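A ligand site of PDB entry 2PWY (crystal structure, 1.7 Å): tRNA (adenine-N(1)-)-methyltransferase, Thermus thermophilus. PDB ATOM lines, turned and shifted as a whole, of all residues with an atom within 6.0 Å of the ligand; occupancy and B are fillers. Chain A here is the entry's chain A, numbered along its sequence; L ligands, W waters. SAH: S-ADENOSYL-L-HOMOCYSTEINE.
O of Thr 105 sits close to OXT of the ligand, at 3.4 Å. Merely in contact with the ligand: Ala 77 (3.7 Å), Thr 78 (3.5 Å), Pro 79 (3.3 Å), Gly 104 (3.3 Å), Gly 106 (3.5 Å), Tyr 127 (3.9 Å), Arg 130 (3.3 Å), Gly 155 (3.5 Å), Lys 156 (3.5 Å), Leu 174 (3.5 Å) and Val 180 (3.8 Å). Of the 31 residues printed, 23 come within 4 Å of the ligand. The nearest printed residue that does not touch the ligand is Ala 103 (4.3 Å).
The side-chain carboxylate (OE1) of Glu 128 is in hydrogen-bond range of an oxygen (O3') of the ligand (2.6 Å). The side-chain carboxylate (OD2) of Asp 173 is in salt-bridge range of a nitrogen (N) of the ligand (2.8 Å). A ring nitrogen (ND1) of His 133 sits at hydrogen-bond distance from an oxygen (O3') of the ligand (2.8 Å). OXT of the ligand is in hydrogen-bond range of N of Ser 107 (2.8 Å). An oxygen (O) of the ligand sits at hydrogen-bond distance from the backbone NH (N) of Thr 80 (2.9 Å). N of the ligand sits at hydrogen-bond distance from OG1 of Thr 80, at 2.8 Å. OE1 of Glu 158 is in hydrogen-bond range of N6 of the ligand (2.8 Å). The backbone NH of Leu 110 sits at hydrogen-bond distance from an oxygen (O) of the ligand (2.9 Å). OXT of the ligand sits at hydrogen-bond distance from N of Gly 108, at 3.1 Å. N of Leu 157 lies within hydrogen-bond range of N1 of the ligand (3.1 Å). The backbone NH (N) of Gly 109 lies within hydrogen-bond range of an oxygen (OXT) of the ligand, at 3.1 Å. N of Ala 129 lies within hydrogen-bond range of N3 of the ligand.
Water W1 lies within hydrogen-bond range of the side-chain carboxylate of Glu 102, the backbone carbonyl oxygen of Gly 104 and a nitrogen (N) of the ligand. Water W3 bridges a nitrogen (N6) of the ligand (2.9 Å) and the backbone carbonyl oxygen of Glu 176 (3.2 Å). Water W5 lies within hydrogen-bond range of N of Glu 176 (2.9 Å), N7 of the ligand (3.0 Å) and N of Met 175 (3.4 Å). Water W4 lies within hydrogen-bond range of OE2 of Glu 102, O of Thr 105, OG1 of Thr 111, N of Leu 110 and N of the ligand.
The side-chain carboxylate of Glu 128 lies within hydrogen-bond range of the backbone NH of Arg 130, at 2.8 Å. OE1 of Glu 128 lies within hydrogen-bond range of N of Thr 105 (3.5 Å). The backbone NH (N) of Gly 106 is in hydrogen-bond range of the side-chain carboxylate (OE1) of Glu 128, 2.8 Å away. OD2 of Asp 173 is in hydrogen-bond range of OG1 of Thr 80, 2.8 Å away. The backbone NH (N) of Gly 104 lies within hydrogen-bond range of the backbone carbonyl oxygen (O) of Asp 173, at 3.0 Å. OG of Ser 107 is in hydrogen-bond range of O of Ala 77. N of Ala 129 sits at hydrogen-bond distance from O of Gly 155, 3.4 Å away. The backbone NH (N) of Thr 105 lies within hydrogen-bond range of the backbone carbonyl oxygen (O) of Tyr 127, 2.9 Å away.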
ATOM      1  N   LEU A  70      39.441  -5.009 -21.218  1.00  0.00           N
ATOM      2  CA  LEU A  70      37.988  -4.892 -20.971  1.00  0.00           C
ATOM      3  C   LEU A  70      37.499  -3.454 -20.985  1.00  0.00           C
ATOM      4  O   LEU A  70      36.415  -3.171 -21.488  1.00  0.00           O
ATOM      5  CB  LEU A  70      37.571  -5.536 -19.647  1.00  0.00           C
ATOM      6  CG  LEU A  70      36.956  -6.920 -19.760  1.00  0.00           C
ATOM      7  CD1 LEU A  70      38.055  -7.913 -20.130  1.00  0.00           C
ATOM      8  CD2 LEU A  70      36.258  -7.315 -18.460  1.00  0.00           C
ATOM      9  N   MET A  73      38.169  -2.165 -25.008  1.00  0.00           N
ATOM     10  CA  MET A  73      37.672  -2.929 -26.157  1.00  0.00           C
ATOM     11  C   MET A  73      36.303  -2.440 -26.641  1.00  0.00           C
ATOM     12  O   MET A  73      35.504  -1.926 -25.847  1.00  0.00           O
ATOM     13  CB  MET A  73      37.622  -4.432 -25.860  1.00  0.00           C
ATOM     14  CG  MET A  73      36.559  -4.843 -24.841  1.00  0.00           C
ATOM     15  SD  MET A  73      36.667  -6.585 -24.422  1.00  0.00           S
ATOM     16  CE  MET A  73      35.133  -6.793 -23.546  1.00  0.00           C
ATOM     17  N   ALA A  77      26.974  -4.804 -25.662  1.00  0.00           N
ATOM     18  CA  ALA A  77      26.661  -4.960 -24.245  1.00  0.00           C
ATOM     19  C   ALA A  77      27.838  -4.497 -23.380  1.00  0.00           C
ATOM     20  O   ALA A  77      28.984  -4.849 -23.649  1.00  0.00           O
ATOM     21  CB  ALA A  77      26.306  -6.400 -23.939  1.00  0.00           C
ATOM     22  N   THR A  78      27.564  -3.702 -22.353  1.00  0.00           N
ATOM     23  CA  THR A  78      28.630  -3.286 -21.429  1.00  0.00           C
ATOM     24  C   THR A  78      29.229  -4.499 -20.693  1.00  0.00           C
ATOM     25  O   THR A  78      28.495  -5.304 -20.099  1.00  0.00           O
ATOM     26  CB  THR A  78      28.140  -2.206 -20.441  1.00  0.00           C
ATOM     27  OG1 THR A  78      27.619  -1.077 -21.177  1.00  0.00           O
ATOM     28  CG2 THR A  78      29.280  -1.733 -19.556  1.00  0.00           C
ATOM     29  N   PRO A  79      30.563  -4.661 -20.759  1.00  0.00           N
ATOM     30  CA  PRO A  79      31.146  -5.825 -20.086  1.00  0.00           C
ATOM     31  C   PRO A  79      31.112  -5.691 -18.574  1.00  0.00           C
ATOM     32  O   PRO A  79      31.051  -4.583 -18.046  1.00  0.00           O
ATOM     33  CB  PRO A  79      32.601  -5.867 -20.572  1.00  0.00           C
ATOM     34  CG  PRO A  79      32.842  -4.604 -21.317  1.00  0.00           C
ATOM     35  CD  PRO A  79      31.579  -3.816 -21.413  1.00  0.00           C
ATOM     36  N   THR A  80      31.182  -6.833 -17.896  1.00  0.00           N
ATOM     37  CA  THR A  80      31.406  -6.887 -16.463  1.00  0.00           C
ATOM     38  C   THR A  80      32.652  -6.072 -16.124  1.00  0.00           C
ATOM     39  O   THR A  80      33.674  -6.184 -16.816  1.00  0.00           O
ATOM     40  CB  THR A  80      31.626  -8.341 -16.025  1.00  0.00           C
ATOM     41  OG1 THR A  80      30.539  -9.155 -16.515  1.00  0.00           O
ATOM     42  CG2 THR A  80      31.734  -8.475 -14.507  1.00  0.00           C
ATOM     43  N   GLU A 102      28.265 -20.093 -18.590  1.00  0.00           N
ATOM     44  CA  GLU A 102      28.109 -18.641 -18.599  1.00  0.00           C
ATOM     45  C   GLU A 102      26.939 -18.179 -19.448  1.00  0.00           C
ATOM     46  O   GLU A 102      26.753 -18.659 -20.566  1.00  0.00           O
ATOM     47  CB  GLU A 102      29.379 -17.939 -19.120  1.00  0.00           C
ATOM     48  CG  GLU A 102      29.229 -16.419 -19.167  1.00  0.00           C
ATOM     49  CD  GLU A 102      30.352 -15.678 -19.907  1.00  0.00           C
ATOM     50  OE1 GLU A 102      30.899 -16.200 -20.910  1.00  0.00           O
ATOM     51  OE2 GLU A 102      30.680 -14.548 -19.481  1.00  0.00           O
ATOM     52  N   ALA A 103      26.174 -17.216 -18.933  1.00  0.00           N
ATOM     53  CA  ALA A 103      25.258 -16.439 -19.777  1.00  0.00           C
ATOM     54  C   ALA A 103      25.034 -15.051 -19.138  1.00  0.00           C
ATOM     55  O   ALA A 103      25.032 -14.954 -17.906  1.00  0.00           O
ATOM     56  CB  ALA A 103      23.921 -17.175 -19.950  1.00  0.00           C
ATOM     57  N   GLY A 104      24.898 -13.982 -19.933  1.00  0.00           N
ATOM     58  CA  GLY A 104      25.086 -14.020 -21.401  1.00  0.00           C
ATOM     59  C   GLY A 104      26.514 -13.635 -21.781  1.00  0.00           C
ATOM     60  O   GLY A 104      27.144 -12.855 -21.062  1.00  0.00           O
ATOM     61  N   THR A 105      27.010 -14.179 -22.892  1.00  0.00           N
ATOM     62  CA  THR A 105      28.380 -13.846 -23.340  1.00  0.00           C
ATOM     63  C   THR A 105      28.600 -12.332 -23.386  1.00  0.00           C
ATOM     64  O   THR A 105      29.665 -11.833 -22.972  1.00  0.00           O
ATOM     65  CB  THR A 105      28.711 -14.483 -24.710  1.00  0.00           C
ATOM     66  OG1 THR A 105      28.199 -15.829 -24.742  1.00  0.00           O
ATOM     67  CG2 THR A 105      30.212 -14.519 -24.954  1.00  0.00           C
ATOM     68  N   GLY A 106      27.599 -11.596 -23.867  1.00  0.00           N
ATOM     69  CA  GLY A 106      27.641 -10.132 -23.889  1.00  0.00           C
ATOM     70  C   GLY A 106      28.691  -9.632 -24.859  1.00  0.00           C
ATOM     71  O   GLY A 106      28.533  -9.772 -26.065  1.00  0.00           O
ATOM     72  N   SER A 107      29.758  -9.028 -24.316  1.00  0.00           N
ATOM     73  CA  SER A 107      30.897  -8.557 -25.117  1.00  0.00           C
ATOM     74  C   SER A 107      32.180  -9.355 -24.848  1.00  0.00           C
ATOM     75  O   SER A 107      33.244  -9.006 -25.329  1.00  0.00           O
ATOM     76  CB  SER A 107      31.127  -7.061 -24.910  1.00  0.00           C
ATOM     77  OG  SER A 107      30.041  -6.345 -25.485  1.00  0.00           O
ATOM     78  N   GLY A 108      32.043 -10.423 -24.063  1.00  0.00           N
ATOM     79  CA  GLY A 108      33.160 -11.334 -23.800  1.00  0.00           C
ATOM     80  C   GLY A 108      34.120 -10.934 -22.690  1.00  0.00           C
ATOM     81  O   GLY A 108      35.162 -11.584 -22.514  1.00  0.00           O
ATOM     82  N   GLY A 109      33.775  -9.916 -21.919  1.00  0.00           N
ATOM     83  CA  GLY A 109      34.671  -9.461 -20.852  1.00  0.00           C
ATOM     84  C   GLY A 109      34.799 -10.511 -19.755  1.00  0.00           C
ATOM     85  O   GLY A 109      35.905 -10.975 -19.458  1.00  0.00           O
ATOM     86  N   LEU A 110      33.673 -10.882 -19.164  1.00  0.00           N
ATOM     87  CA  LEU A 110      33.678 -11.944 -18.141  1.00  0.00           C
ATOM     88  C   LEU A 110      34.183 -13.260 -18.758  1.00  0.00           C
ATOM     89  O   LEU A 110      34.921 -14.009 -18.115  1.00  0.00           O
ATOM     90  CB  LEU A 110      32.292 -12.100 -17.514  1.00  0.00           C
ATOM     91  CG  LEU A 110      32.186 -13.149 -16.404  1.00  0.00           C
ATOM     92  CD1 LEU A 110      33.233 -12.927 -15.320  1.00  0.00           C
ATOM     93  CD2 LEU A 110      30.743 -13.233 -15.822  1.00  0.00           C
ATOM     94  N   THR A 111      33.807 -13.529 -20.015  1.00  0.00           N
ATOM     95  CA  THR A 111      34.278 -14.724 -20.717  1.00  0.00           C
ATOM     96  C   THR A 111      35.797 -14.872 -20.639  1.00  0.00           C
ATOM     97  O   THR A 111      36.310 -15.955 -20.366  1.00  0.00           O
ATOM     98  CB  THR A 111      33.839 -14.737 -22.197  1.00  0.00           C
ATOM     99  OG1 THR A 111      32.431 -14.463 -22.280  1.00  0.00           O
ATOM    100  CG2 THR A 111      34.143 -16.121 -22.813  1.00  0.00           C
ATOM    101  N   TYR A 127      26.688 -18.882 -23.361  1.00  0.00           N
ATOM    102  CA  TYR A 127      25.447 -18.709 -24.147  1.00  0.00           C
ATOM    103  C   TYR A 127      25.123 -17.243 -24.330  1.00  0.00           C
ATOM    104  O   TYR A 127      25.223 -16.458 -23.389  1.00  0.00           O
ATOM    105  CB  TYR A 127      24.255 -19.406 -23.458  1.00  0.00           C
ATOM    106  CG  TYR A 127      24.344 -20.897 -23.618  1.00  0.00           C
ATOM    107  CD1 TYR A 127      23.573 -21.554 -24.560  1.00  0.00           C
ATOM    108  CD2 TYR A 127      25.260 -21.632 -22.854  1.00  0.00           C
ATOM    109  CE1 TYR A 127      23.675 -22.946 -24.726  1.00  0.00           C
ATOM    110  CE2 TYR A 127      25.367 -23.002 -23.030  1.00  0.00           C
ATOM    111  CZ  TYR A 127      24.590 -23.643 -23.962  1.00  0.00           C
ATOM    112  OH  TYR A 127      24.717 -25.008 -24.134  1.00  0.00           O
ATOM    113  N   GLU A 128      24.692 -16.888 -25.541  1.00  0.00           N
ATOM    114  CA  GLU A 128      24.277 -15.528 -25.826  1.00  0.00           C
ATOM    115  C   GLU A 128      23.084 -15.537 -26.784  1.00  0.00           C
ATOM    116  O   GLU A 128      23.187 -16.119 -27.865  1.00  0.00           O
ATOM    117  CB  GLU A 128      25.445 -14.727 -26.420  1.00  0.00           C
ATOM    118  CG  GLU A 128      25.096 -13.348 -26.973  1.00  0.00           C
ATOM    119  CD  GLU A 128      24.405 -12.452 -25.966  1.00  0.00           C
ATOM    120  OE1 GLU A 128      25.006 -12.136 -24.906  1.00  0.00           O
ATOM    121  OE2 GLU A 128      23.256 -12.032 -26.242  1.00  0.00           O
ATOM    122  N   ALA A 129      21.987 -14.882 -26.387  1.00  0.00           N
ATOM    123  CA  ALA A 129      20.731 -14.876 -27.164  1.00  0.00           C
ATOM    124  C   ALA A 129      20.772 -13.974 -28.393  1.00  0.00           C
ATOM    125  O   ALA A 129      20.067 -14.227 -29.382  1.00  0.00           O
ATOM    126  CB  ALA A 129      19.568 -14.465 -26.265  1.00  0.00           C
ATOM    127  N   ARG A 130      21.575 -12.911 -28.336  1.00  0.00           N
ATOM    128  CA  ARG A 130      21.567 -11.895 -29.390  1.00  0.00           C
ATOM    129  C   ARG A 130      22.757 -12.050 -30.347  1.00  0.00           C
ATOM    130  O   ARG A 130      23.903 -11.937 -29.919  1.00  0.00           O
ATOM    131  CB  ARG A 130      21.535 -10.499 -28.779  1.00  0.00           C
ATOM    132  CG  ARG A 130      20.277 -10.222 -27.965  1.00  0.00           C
ATOM    133  CD  ARG A 130      20.287  -8.845 -27.321  1.00  0.00           C
ATOM    134  NE  ARG A 130      20.223  -7.772 -28.322  1.00  0.00           N
ATOM    135  CZ  ARG A 130      20.030  -6.489 -28.032  1.00  0.00           C
ATOM    136  NH1 ARG A 130      19.871  -6.092 -26.771  1.00  0.00           N
ATOM    137  NH2 ARG A 130      19.985  -5.595 -29.022  1.00  0.00           N
ATOM    138  N   HIS A 133      25.478  -9.263 -30.546  1.00  0.00           N
ATOM    139  CA  HIS A 133      26.245  -9.307 -29.313  1.00  0.00           C
ATOM    140  C   HIS A 133      27.263 -10.438 -29.361  1.00  0.00           C
ATOM    141  O   HIS A 133      28.444 -10.227 -29.074  1.00  0.00           O
ATOM    142  CB  HIS A 133      25.323  -9.443 -28.093  1.00  0.00           C
ATOM    143  CG  HIS A 133      24.553  -8.196 -27.751  1.00  0.00           C
ATOM    144  ND1 HIS A 133      23.945  -8.008 -26.522  1.00  0.00           N
ATOM    145  CD2 HIS A 133      24.286  -7.079 -28.470  1.00  0.00           C
ATOM    146  CE1 HIS A 133      23.349  -6.830 -26.499  1.00  0.00           C
ATOM    147  NE2 HIS A 133      23.548  -6.240 -27.668  1.00  0.00           N
ATOM    148  N   GLY A 155      21.836 -18.575 -28.538  1.00  0.00           N
ATOM    149  CA  GLY A 155      20.551 -19.023 -28.003  1.00  0.00           C
ATOM    150  C   GLY A 155      20.362 -18.659 -26.545  1.00  0.00           C
ATOM    151  O   GLY A 155      21.285 -18.201 -25.876  1.00  0.00           O
ATOM    152  N   LYS A 156      19.143 -18.871 -26.073  1.00  0.00           N
ATOM    153  CA  LYS A 156      18.812 -18.639 -24.673  1.00  0.00           C
ATOM    154  C   LYS A 156      19.313 -19.793 -23.820  1.00  0.00           C
ATOM    155  O   LYS A 156      19.171 -20.968 -24.202  1.00  0.00           O
ATOM    156  CB  LYS A 156      17.309 -18.459 -24.490  1.00  0.00           C
ATOM    157  CG  LYS A 156      16.756 -17.199 -25.136  1.00  0.00           C
ATOM    158  CD  LYS A 156      15.248 -17.280 -25.320  1.00  0.00           C
ATOM    159  CE  LYS A 156      14.681 -16.025 -26.005  1.00  0.00           C
ATOM    160  NZ  LYS A 156      15.362 -15.704 -27.318  1.00  0.00           N
ATOM    161  N   LEU A 157      19.911 -19.474 -22.673  1.00  0.00           N
ATOM    162  CA  LEU A 157      20.374 -20.497 -21.755  1.00  0.00           C
ATOM    163  C   LEU A 157      19.205 -21.419 -21.338  1.00  0.00           C
ATOM    164  O   LEU A 157      19.418 -22.621 -21.214  1.00  0.00           O
ATOM    165  CB  LEU A 157      21.063 -19.879 -20.545  1.00  0.00           C
ATOM    166  CG  LEU A 157      21.640 -20.857 -19.494  1.00  0.00           C
ATOM    167  CD1 LEU A 157      22.615 -21.856 -20.151  1.00  0.00           C
ATOM    168  CD2 LEU A 157      22.304 -20.134 -18.321  1.00  0.00           C
ATOM    169  N   GLU A 158      18.003 -20.858 -21.180  1.00  0.00           N
ATOM    170  CA  GLU A 158      16.785 -21.624 -20.813  1.00  0.00           C
ATOM    171  C   GLU A 158      16.553 -22.838 -21.710  1.00  0.00           C
ATOM    172  O   GLU A 158      15.891 -23.792 -21.304  1.00  0.00           O
ATOM    173  CB  GLU A 158      15.512 -20.776 -20.965  1.00  0.00           C
ATOM    174  CG  GLU A 158      15.343 -19.637 -20.062  1.00  0.00           C
ATOM    175  CD  GLU A 158      15.894 -18.362 -20.645  1.00  0.00           C
ATOM    176  OE1 GLU A 158      17.058 -18.362 -21.101  1.00  0.00           O
ATOM    177  OE2 GLU A 158      15.166 -17.351 -20.607  1.00  0.00           O
ATOM    178  N   ASP A 173      25.535 -13.036 -15.925  1.00  0.00           N
ATOM    179  CA  ASP A 173      25.443 -11.590 -16.072  1.00  0.00           C
ATOM    180  C   ASP A 173      24.347 -11.357 -17.103  1.00  0.00           C
ATOM    181  O   ASP A 173      24.591 -11.434 -18.298  1.00  0.00           O
ATOM    182  CB  ASP A 173      26.785 -10.988 -16.519  1.00  0.00           C
ATOM    183  CG  ASP A 173      26.712  -9.473 -16.718  1.00  0.00           C
ATOM    184  OD1 ASP A 173      25.620  -8.865 -16.546  1.00  0.00           O
ATOM    185  OD2 ASP A 173      27.760  -8.884 -17.075  1.00  0.00           O
ATOM    186  N   LEU A 174      23.139 -11.127 -16.599  1.00  0.00           N
ATOM    187  CA  LEU A 174      21.946 -10.915 -17.433  1.00  0.00           C
ATOM    188  C   LEU A 174      20.829 -10.326 -16.562  1.00  0.00           C
ATOM    189  O   LEU A 174      20.876 -10.426 -15.331  1.00  0.00           O
ATOM    190  CB  LEU A 174      21.510 -12.204 -18.154  1.00  0.00           C
ATOM    191  CG  LEU A 174      21.726 -13.601 -17.522  1.00  0.00           C
ATOM    192  CD1 LEU A 174      20.907 -13.720 -16.248  1.00  0.00           C
ATOM    193  CD2 LEU A 174      21.380 -14.754 -18.481  1.00  0.00           C
ATOM    194  N   MET A 175      19.838  -9.713 -17.211  1.00  0.00           N
ATOM    195  CA  MET A 175      18.830  -8.909 -16.514  1.00  0.00           C
ATOM    196  C   MET A 175      17.875  -9.739 -15.661  1.00  0.00           C
ATOM    197  O   MET A 175      17.399  -9.259 -14.629  1.00  0.00           O
ATOM    198  CB  MET A 175      18.005  -8.107 -17.526  1.00  0.00           C
ATOM    199  N   GLU A 176      17.577 -10.966 -16.094  1.00  0.00           N
ATOM    200  CA  GLU A 176      16.554 -11.784 -15.446  1.00  0.00           C
ATOM    201  C   GLU A 176      17.065 -13.191 -15.148  1.00  0.00           C
ATOM    202  O   GLU A 176      16.608 -14.178 -15.762  1.00  0.00           O
ATOM    203  CB  GLU A 176      15.299 -11.842 -16.313  1.00  0.00           C
ATOM    204  CG  GLU A 176      14.701 -10.469 -16.593  1.00  0.00           C
ATOM    205  CD  GLU A 176      13.543 -10.497 -17.541  1.00  0.00           C
ATOM    206  OE1 GLU A 176      13.680 -11.075 -18.646  1.00  0.00           O
ATOM    207  OE2 GLU A 176      12.491  -9.941 -17.178  1.00  0.00           O
ATOM    208  N   LYS A 179      15.011 -16.547 -14.606  1.00  0.00           N
ATOM    209  CA  LYS A 179      14.553 -17.342 -15.742  1.00  0.00           C
ATOM    210  C   LYS A 179      15.438 -18.535 -16.114  1.00  0.00           C
ATOM    211  O   LYS A 179      14.983 -19.462 -16.796  1.00  0.00           O
ATOM    212  CB  LYS A 179      14.361 -16.466 -16.976  1.00  0.00           C
ATOM    213  CG  LYS A 179      13.231 -15.460 -16.849  1.00  0.00           C
ATOM    214  CD  LYS A 179      12.953 -14.804 -18.202  1.00  0.00           C
ATOM    215  CE  LYS A 179      11.971 -13.650 -18.092  1.00  0.00           C
ATOM    216  NZ  LYS A 179      10.838 -13.910 -17.185  1.00  0.00           N
ATOM    217  N   VAL A 180      16.695 -18.522 -15.662  1.00  0.00           N
ATOM    218  CA  VAL A 180      17.672 -19.574 -16.017  1.00  0.00           C
ATOM    219  C   VAL A 180      18.043 -20.464 -14.825  1.00  0.00           C
ATOM    220  O   VAL A 180      18.943 -21.310 -14.930  1.00  0.00           O
ATOM    221  CB  VAL A 180      18.951 -18.990 -16.714  1.00  0.00           C
ATOM    222  CG1 VAL A 180      18.584 -18.172 -17.930  1.00  0.00           C
ATOM    223  CG2 VAL A 180      19.814 -18.156 -15.753  1.00  0.00           C
HETATM  224  N   SAH L   1      29.364 -10.324 -18.805  1.00  0.00           N
HETATM  225  CA  SAH L   1      29.274  -9.816 -20.207  1.00  0.00           C
HETATM  226  CB  SAH L   1      28.137  -8.821 -20.363  1.00  0.00           C
HETATM  227  CG  SAH L   1      26.768  -9.498 -20.362  1.00  0.00           C
HETATM  228  SD  SAH L   1      25.486  -8.292 -20.816  1.00  0.00           S
HETATM  229  C   SAH L   1      30.612  -9.200 -20.583  1.00  0.00           C
HETATM  230  O   SAH L   1      31.489  -9.077 -19.714  1.00  0.00           O
HETATM  231  OXT SAH L   1      30.835  -8.839 -21.738  1.00  0.00           O
HETATM  232  C5' SAH L   1      24.101  -9.449 -20.739  1.00  0.00           C
HETATM  233  C4' SAH L   1      23.974 -10.293 -22.019  1.00  0.00           C
HETATM  234  O4' SAH L   1      23.159 -11.413 -21.740  1.00  0.00           O
HETATM  235  C3' SAH L   1      23.328  -9.579 -23.208  1.00  0.00           C
HETATM  236  O3' SAH L   1      24.199  -9.712 -24.328  1.00  0.00           O
HETATM  237  C2' SAH L   1      22.006 -10.306 -23.423  1.00  0.00           C
HETATM  238  O2' SAH L   1      21.649 -10.443 -24.786  1.00  0.00           O
HETATM  239  C1' SAH L   1      22.307 -11.673 -22.860  1.00  0.00           C
HETATM  240  N9  SAH L   1      21.201 -12.455 -22.292  1.00  0.00           N
HETATM  241  C8  SAH L   1      20.245 -12.013 -21.431  1.00  0.00           C
HETATM  242  N7  SAH L   1      19.479 -13.077 -21.093  1.00  0.00           N
HETATM  243  C5  SAH L   1      19.961 -14.185 -21.690  1.00  0.00           C
HETATM  244  C6  SAH L   1      19.559 -15.531 -21.679  1.00  0.00           C
HETATM  245  N6  SAH L   1      18.495 -15.931 -20.955  1.00  0.00           N
HETATM  246  N1  SAH L   1      20.288 -16.435 -22.429  1.00  0.00           N
HETATM  247  C2  SAH L   1      21.376 -16.039 -23.170  1.00  0.00           C
HETATM  248  N3  SAH L   1      21.751 -14.708 -23.177  1.00  0.00           N
HETATM  249  C4  SAH L   1      21.056 -13.805 -22.441  1.00  0.00           C
HETATM  250  O   HOH W   1      28.568 -12.979 -18.699  1.00  0.00           O
HETATM  251  O   HOH W   2      18.978 -11.194 -24.673  1.00  0.00           O
HETATM  252  O   HOH W   3      16.802 -14.723 -18.942  1.00  0.00           O
HETATM  253  O   HOH W   4      31.223 -12.240 -20.733  1.00  0.00           O
HETATM  254  O   HOH W   5      17.845 -11.983 -18.823  1.00  0.00           O
HETATM  255  O   HOH W   6      20.161  -9.074 -20.159  1.00  0.00           O
